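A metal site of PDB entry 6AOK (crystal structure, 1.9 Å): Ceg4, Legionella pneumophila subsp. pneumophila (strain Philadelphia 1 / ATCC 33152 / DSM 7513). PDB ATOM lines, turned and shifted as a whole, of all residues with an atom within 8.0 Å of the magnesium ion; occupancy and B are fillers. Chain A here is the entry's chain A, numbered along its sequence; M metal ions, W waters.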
ATOM      1  N   THR A  17      -2.291  35.309   4.018  1.00  0.00           N
ATOM      2  CA  THR A  17      -1.137  34.723   4.671  1.00  0.00           C
ATOM      3  C   THR A  17      -1.594  33.564   5.553  1.00  0.00           C
ATOM      4  O   THR A  17      -2.620  33.644   6.237  1.00  0.00           O
ATOM      5  CB  THR A  17      -0.374  35.764   5.520  1.00  0.00           C
ATOM      6  OG1 THR A  17       0.754  35.140   6.120  1.00  0.00           O
ATOM      7  CG2 THR A  17      -1.243  36.320   6.607  1.00  0.00           C
ATOM      8  N   ASP A  18      -0.851  32.481   5.499  1.00  0.00           N
ATOM      9  CA  ASP A  18      -0.952  31.413   6.479  1.00  0.00           C
ATOM     10  C   ASP A  18      -0.575  31.945   7.876  1.00  0.00           C
ATOM     11  O   ASP A  18       0.032  33.014   8.019  1.00  0.00           O
ATOM     12  CB  ASP A  18      -0.016  30.266   6.051  1.00  0.00           C
ATOM     13  CG  ASP A  18      -0.078  29.072   6.996  1.00  0.00           C
ATOM     14  OD1 ASP A  18      -1.208  28.652   7.385  1.00  0.00           O
ATOM     15  OD2 ASP A  18       1.013  28.556   7.334  1.00  0.00           O
ATOM     16  N   PHE A  19      -0.962  31.204   8.921  1.00  0.00           N
ATOM     17  CA  PHE A  19      -0.542  31.575  10.274  1.00  0.00           C
ATOM     18  C   PHE A  19       0.592  30.681  10.770  1.00  0.00           C
ATOM     19  O   PHE A  19       1.741  31.136  10.848  1.00  0.00           O
ATOM     20  CB  PHE A  19      -1.756  31.576  11.246  1.00  0.00           C
ATOM     21  CG  PHE A  19      -1.384  32.020  12.646  1.00  0.00           C
ATOM     22  CD1 PHE A  19      -1.154  33.377  12.911  1.00  0.00           C
ATOM     23  CD2 PHE A  19      -1.275  31.095  13.684  1.00  0.00           C
ATOM     24  CE1 PHE A  19      -0.805  33.801  14.186  1.00  0.00           C
ATOM     25  CE2 PHE A  19      -0.920  31.524  14.971  1.00  0.00           C
ATOM     26  CZ  PHE A  19      -0.689  32.870  15.206  1.00  0.00           C
ATOM     27  N   ASP A  20       0.322  29.405  11.091  1.00  0.00           N
ATOM     28  CA  ASP A  20       1.321  28.556  11.744  1.00  0.00           C
ATOM     29  C   ASP A  20       2.442  28.223  10.785  1.00  0.00           C
ATOM     30  O   ASP A  20       2.190  27.601   9.733  1.00  0.00           O
ATOM     31  CB  ASP A  20       0.683  27.241  12.214  1.00  0.00           C
ATOM     32  CG  ASP A  20      -0.391  27.443  13.233  1.00  0.00           C
ATOM     33  OD1 ASP A  20      -0.112  27.939  14.369  1.00  0.00           O
ATOM     34  OD2 ASP A  20      -1.549  27.121  12.887  1.00  0.00           O
ATOM     35  N   GLY A  21       3.683  28.556  11.171  1.00  0.00           N
ATOM     36  CA  GLY A  21       4.825  28.271  10.350  1.00  0.00           C
ATOM     37  C   GLY A  21       5.092  29.332   9.292  1.00  0.00           C
ATOM     38  O   GLY A  21       6.092  29.249   8.587  1.00  0.00           O
ATOM     39  N   THR A  22       4.219  30.322   9.179  1.00  0.00           N
ATOM     40  CA  THR A  22       4.437  31.451   8.292  1.00  0.00           C
ATOM     41  C   THR A  22       4.590  32.711   9.128  1.00  0.00           C
ATOM     42  O   THR A  22       5.673  33.320   9.186  1.00  0.00           O
ATOM     43  CB  THR A  22       3.248  31.526   7.306  1.00  0.00           C
ATOM     44  OG1 THR A  22       3.215  30.305   6.505  1.00  0.00           O
ATOM     45  CG2 THR A  22       3.374  32.759   6.396  1.00  0.00           C
ATOM     46  N   VAL A  23       3.526  33.104   9.822  1.00  0.00           N
ATOM     47  CA  VAL A  23       3.631  34.158  10.826  1.00  0.00           C
ATOM     48  C   VAL A  23       4.385  33.647  12.072  1.00  0.00           C
ATOM     49  O   VAL A  23       5.214  34.359  12.637  1.00  0.00           O
ATOM     50  CB  VAL A  23       2.223  34.681  11.168  1.00  0.00           C
ATOM     51  CG1 VAL A  23       2.275  35.691  12.255  1.00  0.00           C
ATOM     52  CG2 VAL A  23       1.504  35.346   9.931  1.00  0.00           C
ATOM     53  N   THR A  24       4.137  32.407  12.502  1.00  0.00           N
ATOM     54  CA  THR A  24       4.876  31.820  13.620  1.00  0.00           C
ATOM     55  C   THR A  24       6.024  31.009  13.101  1.00  0.00           C
ATOM     56  O   THR A  24       6.139  30.767  11.903  1.00  0.00           O
ATOM     57  CB  THR A  24       4.014  30.923  14.520  1.00  0.00           C
ATOM     58  OG1 THR A  24       3.816  29.648  13.862  1.00  0.00           O
ATOM     59  CG2 THR A  24       2.734  31.549  14.834  1.00  0.00           C
ATOM     60  N   LYS A  26       6.489  27.690  13.936  1.00  0.00           N
ATOM     61  CA  LYS A  26       6.210  26.266  14.110  1.00  0.00           C
ATOM     62  C   LYS A  26       5.038  25.915  13.198  1.00  0.00           C
ATOM     63  O   LYS A  26       4.026  26.619  13.210  1.00  0.00           O
ATOM     64  CB  LYS A  26       5.835  25.933  15.567  1.00  0.00           C
ATOM     65  CG  LYS A  26       6.999  25.742  16.469  1.00  0.00           C
ATOM     66  CD  LYS A  26       7.789  24.486  16.063  1.00  0.00           C
ATOM     67  CE  LYS A  26       8.976  24.219  17.009  1.00  0.00           C
ATOM     68  NZ  LYS A  26      10.054  25.272  16.892  1.00  0.00           N
ATOM     69  N   SER A  27       5.150  24.796  12.498  1.00  0.00           N
ATOM     70  CA  SER A  27       4.061  24.341  11.640  1.00  0.00           C
ATOM     71  C   SER A  27       2.816  23.942  12.447  1.00  0.00           C
ATOM     72  O   SER A  27       2.863  23.664  13.659  1.00  0.00           O
ATOM     73  CB  SER A  27       4.522  23.140  10.800  1.00  0.00           C
ATOM     74  OG  SER A  27       4.556  21.994  11.621  1.00  0.00           O
ATOM     75  N   GLY A  28       1.674  23.905  11.760  1.00  0.00           N
ATOM     76  CA  GLY A  28       0.412  23.605  12.440  1.00  0.00           C
ATOM     77  C   GLY A  28       0.425  22.311  13.233  1.00  0.00           C
ATOM     78  O   GLY A  28       0.028  22.274  14.399  1.00  0.00           O
ATOM     79  N   ASN A  29       0.898  21.221  12.608  1.00  0.00           N
ATOM     80  CA  ASN A  29       0.826  19.985  13.372  1.00  0.00           C
ATOM     81  C   ASN A  29       1.924  19.864  14.427  1.00  0.00           C
ATOM     82  O   ASN A  29       1.869  18.946  15.265  1.00  0.00           O
ATOM     83  CB  ASN A  29       0.787  18.762  12.402  1.00  0.00           C
ATOM     84  CG  ASN A  29       2.122  18.336  11.901  1.00  0.00           C
ATOM     85  OD1 ASN A  29       3.090  19.090  11.970  1.00  0.00           O
ATOM     86  ND2 ASN A  29       2.179  17.119  11.312  1.00  0.00           N
ATOM     87  N   VAL A 111      -5.430  32.854   6.406  1.00  0.00           N
ATOM     88  CA  VAL A 111      -6.156  31.687   5.912  1.00  0.00           C
ATOM     89  C   VAL A 111      -5.500  30.466   6.551  1.00  0.00           C
ATOM     90  O   VAL A 111      -4.307  30.242   6.356  1.00  0.00           O
ATOM     91  CB  VAL A 111      -6.095  31.601   4.387  1.00  0.00           C
ATOM     92  CG1 VAL A 111      -7.019  30.534   3.864  1.00  0.00           C
ATOM     93  CG2 VAL A 111      -6.376  33.049   3.710  1.00  0.00           C
ATOM     94  N   THR A 112      -6.269  29.690   7.291  1.00  0.00           N
ATOM     95  CA  THR A 112      -5.619  28.838   8.258  1.00  0.00           C
ATOM     96  C   THR A 112      -6.439  27.573   8.508  1.00  0.00           C
ATOM     97  O   THR A 112      -7.659  27.567   8.329  1.00  0.00           O
ATOM     98  CB  THR A 112      -5.426  29.656   9.561  1.00  0.00           C
ATOM     99  OG1 THR A 112      -4.647  28.917  10.442  1.00  0.00           O
ATOM    100  CG2 THR A 112      -6.787  29.978  10.230  1.00  0.00           C
ATOM    101  N   LYS A 113      -5.793  26.533   8.973  1.00  0.00           N
ATOM    102  CA  LYS A 113      -6.536  25.415   9.553  1.00  0.00           C
ATOM    103  C   LYS A 113      -6.502  25.477  11.078  1.00  0.00           C
ATOM    104  O   LYS A 113      -6.978  24.528  11.752  1.00  0.00           O
ATOM    105  CB  LYS A 113      -5.974  24.076   9.086  1.00  0.00           C
ATOM    106  CG  LYS A 113      -6.098  23.845   7.569  1.00  0.00           C
ATOM    107  CD  LYS A 113      -5.171  22.730   7.060  1.00  0.00           C
ATOM    108  CE  LYS A 113      -5.006  23.020   5.547  1.00  0.00           C
ATOM    109  NZ  LYS A 113      -4.144  22.069   4.850  1.00  0.00           N
ATOM    110  N   LYS A 144      -8.168  26.137   1.655  1.00  0.00           N
ATOM    111  CA  LYS A 144      -7.675  27.479   1.355  1.00  0.00           C
ATOM    112  C   LYS A 144      -8.123  27.969  -0.023  1.00  0.00           C
ATOM    113  O   LYS A 144      -8.354  29.179  -0.192  1.00  0.00           O
ATOM    114  CB  LYS A 144      -6.149  27.495   1.482  1.00  0.00           C
ATOM    115  CG  LYS A 144      -5.693  27.163   2.925  1.00  0.00           C
ATOM    116  CD  LYS A 144      -4.344  27.868   3.279  1.00  0.00           C
ATOM    117  CE  LYS A 144      -3.870  27.411   4.646  1.00  0.00           C
ATOM    118  NZ  LYS A 144      -2.597  28.065   5.133  1.00  0.00           N
ATOM    119  N   LEU A 165       1.415  34.057   1.207  1.00  0.00           N
ATOM    120  CA  LEU A 165       2.495  33.539   2.045  1.00  0.00           C
ATOM    121  C   LEU A 165       2.046  32.236   2.640  1.00  0.00           C
ATOM    122  O   LEU A 165       0.984  32.193   3.282  1.00  0.00           O
ATOM    123  CB  LEU A 165       2.860  34.521   3.173  1.00  0.00           C
ATOM    124  CG  LEU A 165       3.298  35.848   2.588  1.00  0.00           C
ATOM    125  CD1 LEU A 165       2.166  36.840   2.810  1.00  0.00           C
ATOM    126  CD2 LEU A 165       4.606  36.357   3.190  1.00  0.00           C
ATOM    127  N   ASP A 166       2.820  31.180   2.445  1.00  0.00           N
ATOM    128  CA  ASP A 166       2.458  29.903   3.088  1.00  0.00           C
ATOM    129  C   ASP A 166       3.674  28.989   3.130  1.00  0.00           C
ATOM    130  O   ASP A 166       4.428  28.901   2.153  1.00  0.00           O
ATOM    131  CB  ASP A 166       1.293  29.213   2.341  1.00  0.00           C
ATOM    132  CG  ASP A 166       0.486  28.283   3.238  1.00  0.00           C
ATOM    133  OD1 ASP A 166       1.110  27.467   3.949  1.00  0.00           O
ATOM    134  OD2 ASP A 166      -0.788  28.346   3.207  1.00  0.00           O
ATOM    135  N   ASP A 167       3.870  28.318   4.267  1.00  0.00           N
ATOM    136  CA  ASP A 167       4.961  27.363   4.297  1.00  0.00           C
ATOM    137  C   ASP A 167       4.593  25.998   3.725  1.00  0.00           C
ATOM    138  O   ASP A 167       5.495  25.193   3.489  1.00  0.00           O
ATOM    139  CB  ASP A 167       5.521  27.176   5.746  1.00  0.00           C
ATOM    140  CG  ASP A 167       4.469  26.574   6.714  1.00  0.00           C
ATOM    141  OD1 ASP A 167       3.350  27.136   6.841  1.00  0.00           O
ATOM    142  OD2 ASP A 167       4.730  25.524   7.358  1.00  0.00           O
ATOM    143  N   SER A 168       3.334  25.706   3.509  1.00  0.00           N
ATOM    144  CA  SER A 168       2.936  24.441   2.927  1.00  0.00           C
ATOM    145  C   SER A 168       2.826  24.575   1.412  1.00  0.00           C
ATOM    146  O   SER A 168       2.006  25.347   0.941  1.00  0.00           O
ATOM    147  CB  SER A 168       1.590  24.011   3.514  1.00  0.00           C
ATOM    148  OG  SER A 168       0.914  23.161   2.605  1.00  0.00           O
ATOM    149  N   ASP A 171      -0.902  24.088   0.113  1.00  0.00           N
ATOM    150  CA  ASP A 171      -1.807  25.176   0.460  1.00  0.00           C
ATOM    151  C   ASP A 171      -1.447  26.465  -0.265  1.00  0.00           C
ATOM    152  O   ASP A 171      -2.322  27.186  -0.753  1.00  0.00           O
ATOM    153  CB  ASP A 171      -1.835  25.375   1.973  1.00  0.00           C
ATOM    154  CG  ASP A 171      -2.500  24.180   2.708  1.00  0.00           C
ATOM    155  OD1 ASP A 171      -3.647  23.836   2.384  1.00  0.00           O
ATOM    156  OD2 ASP A 171      -1.877  23.604   3.610  1.00  0.00           O
ATOM    157  N   LYS A 194       7.974  29.658   1.765  1.00  0.00           N
ATOM    158  CA  LYS A 194       9.218  29.504   2.496  1.00  0.00           C
ATOM    159  C   LYS A 194       9.005  28.473   3.599  1.00  0.00           C
ATOM    160  O   LYS A 194       7.878  28.211   4.028  1.00  0.00           O
ATOM    161  CB  LYS A 194       9.680  30.856   3.097  1.00  0.00           C
ATOM    162  CG  LYS A 194       9.759  31.988   2.123  1.00  0.00           C
ATOM    163  CD  LYS A 194      10.715  31.637   1.038  1.00  0.00           C
ATOM    164  CE  LYS A 194      11.116  32.854   0.251  1.00  0.00           C
ATOM    165  NZ  LYS A 194      12.154  32.498  -0.778  1.00  0.00           N
ATOM    166  N   PRO A 196       9.370  27.432   7.644  1.00  0.00           N
ATOM    167  CA  PRO A 196       9.188  28.237   8.862  1.00  0.00           C
ATOM    168  C   PRO A 196      10.473  28.919   9.277  1.00  0.00           C
ATOM    169  O   PRO A 196      11.552  28.363   9.132  1.00  0.00           O
ATOM    170  CB  PRO A 196       8.740  27.210   9.907  1.00  0.00           C
ATOM    171  CG  PRO A 196       7.978  26.153   9.074  1.00  0.00           C
ATOM    172  CD  PRO A 196       8.746  26.094   7.746  1.00  0.00           C
ATOM    173  N   PHE A 199      10.659  33.352   6.209  1.00  0.00           N
ATOM    174  CA  PHE A 199       9.986  34.486   5.580  1.00  0.00           C
ATOM    175  C   PHE A 199      10.652  35.799   6.004  1.00  0.00           C
ATOM    176  O   PHE A 199      10.878  36.025   7.205  1.00  0.00           O
ATOM    177  CB  PHE A 199       8.520  34.500   5.970  1.00  0.00           C
ATOM    178  CG  PHE A 199       7.731  33.365   5.397  1.00  0.00           C
ATOM    179  CD1 PHE A 199       7.638  32.135   6.073  1.00  0.00           C
ATOM    180  CD2 PHE A 199       7.111  33.499   4.177  1.00  0.00           C
ATOM    181  CE1 PHE A 199       6.885  31.063   5.528  1.00  0.00           C
ATOM    182  CE2 PHE A 199       6.372  32.412   3.642  1.00  0.00           C
ATOM    183  CZ  PHE A 199       6.259  31.220   4.343  1.00  0.00           C
HETATM  184 MG    MG M   1       1.617  26.785   7.969  1.00  0.00          MG
HETATM  185  O   HOH W   1       0.834  26.010   6.168  1.00  0.00           O
HETATM  186  O   HOH W   2      -0.154  26.113   8.749  1.00  0.00           O
HETATM  187  O   HOH W   3       2.586  24.983   8.499  1.00  0.00           O
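OG1 of Thr 22 lies within hydrogen-bond range of N of Asp 167 (3.1 Å). The side-chain amino group of Lys 144 is in salt-bridge range of the side-chain carboxylate of Asp 18 (2.7 Å). The backbone carbonyl oxygen of Leu 165 is in hydrogen-bond range of the backbone NH of Asp 18, 2.9 Å away. The side-chain carboxylate of Asp 18 sits close to the side-chain hydroxyl of Thr 22.
The magnesium ion is bound by the side-chain carboxylate (OD2) of Asp 18 (2.0 Å), the backbone carbonyl oxygen (O) of Asp 20 (2.0 Å), water W2 (2.0 Å), the side-chain carboxylate (OD1) of Asp 167 (2.1 Å), water W1 (2.1 Å) and water W3 (2.1 Å). The magnesium ion has six donor atoms within binding distance.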
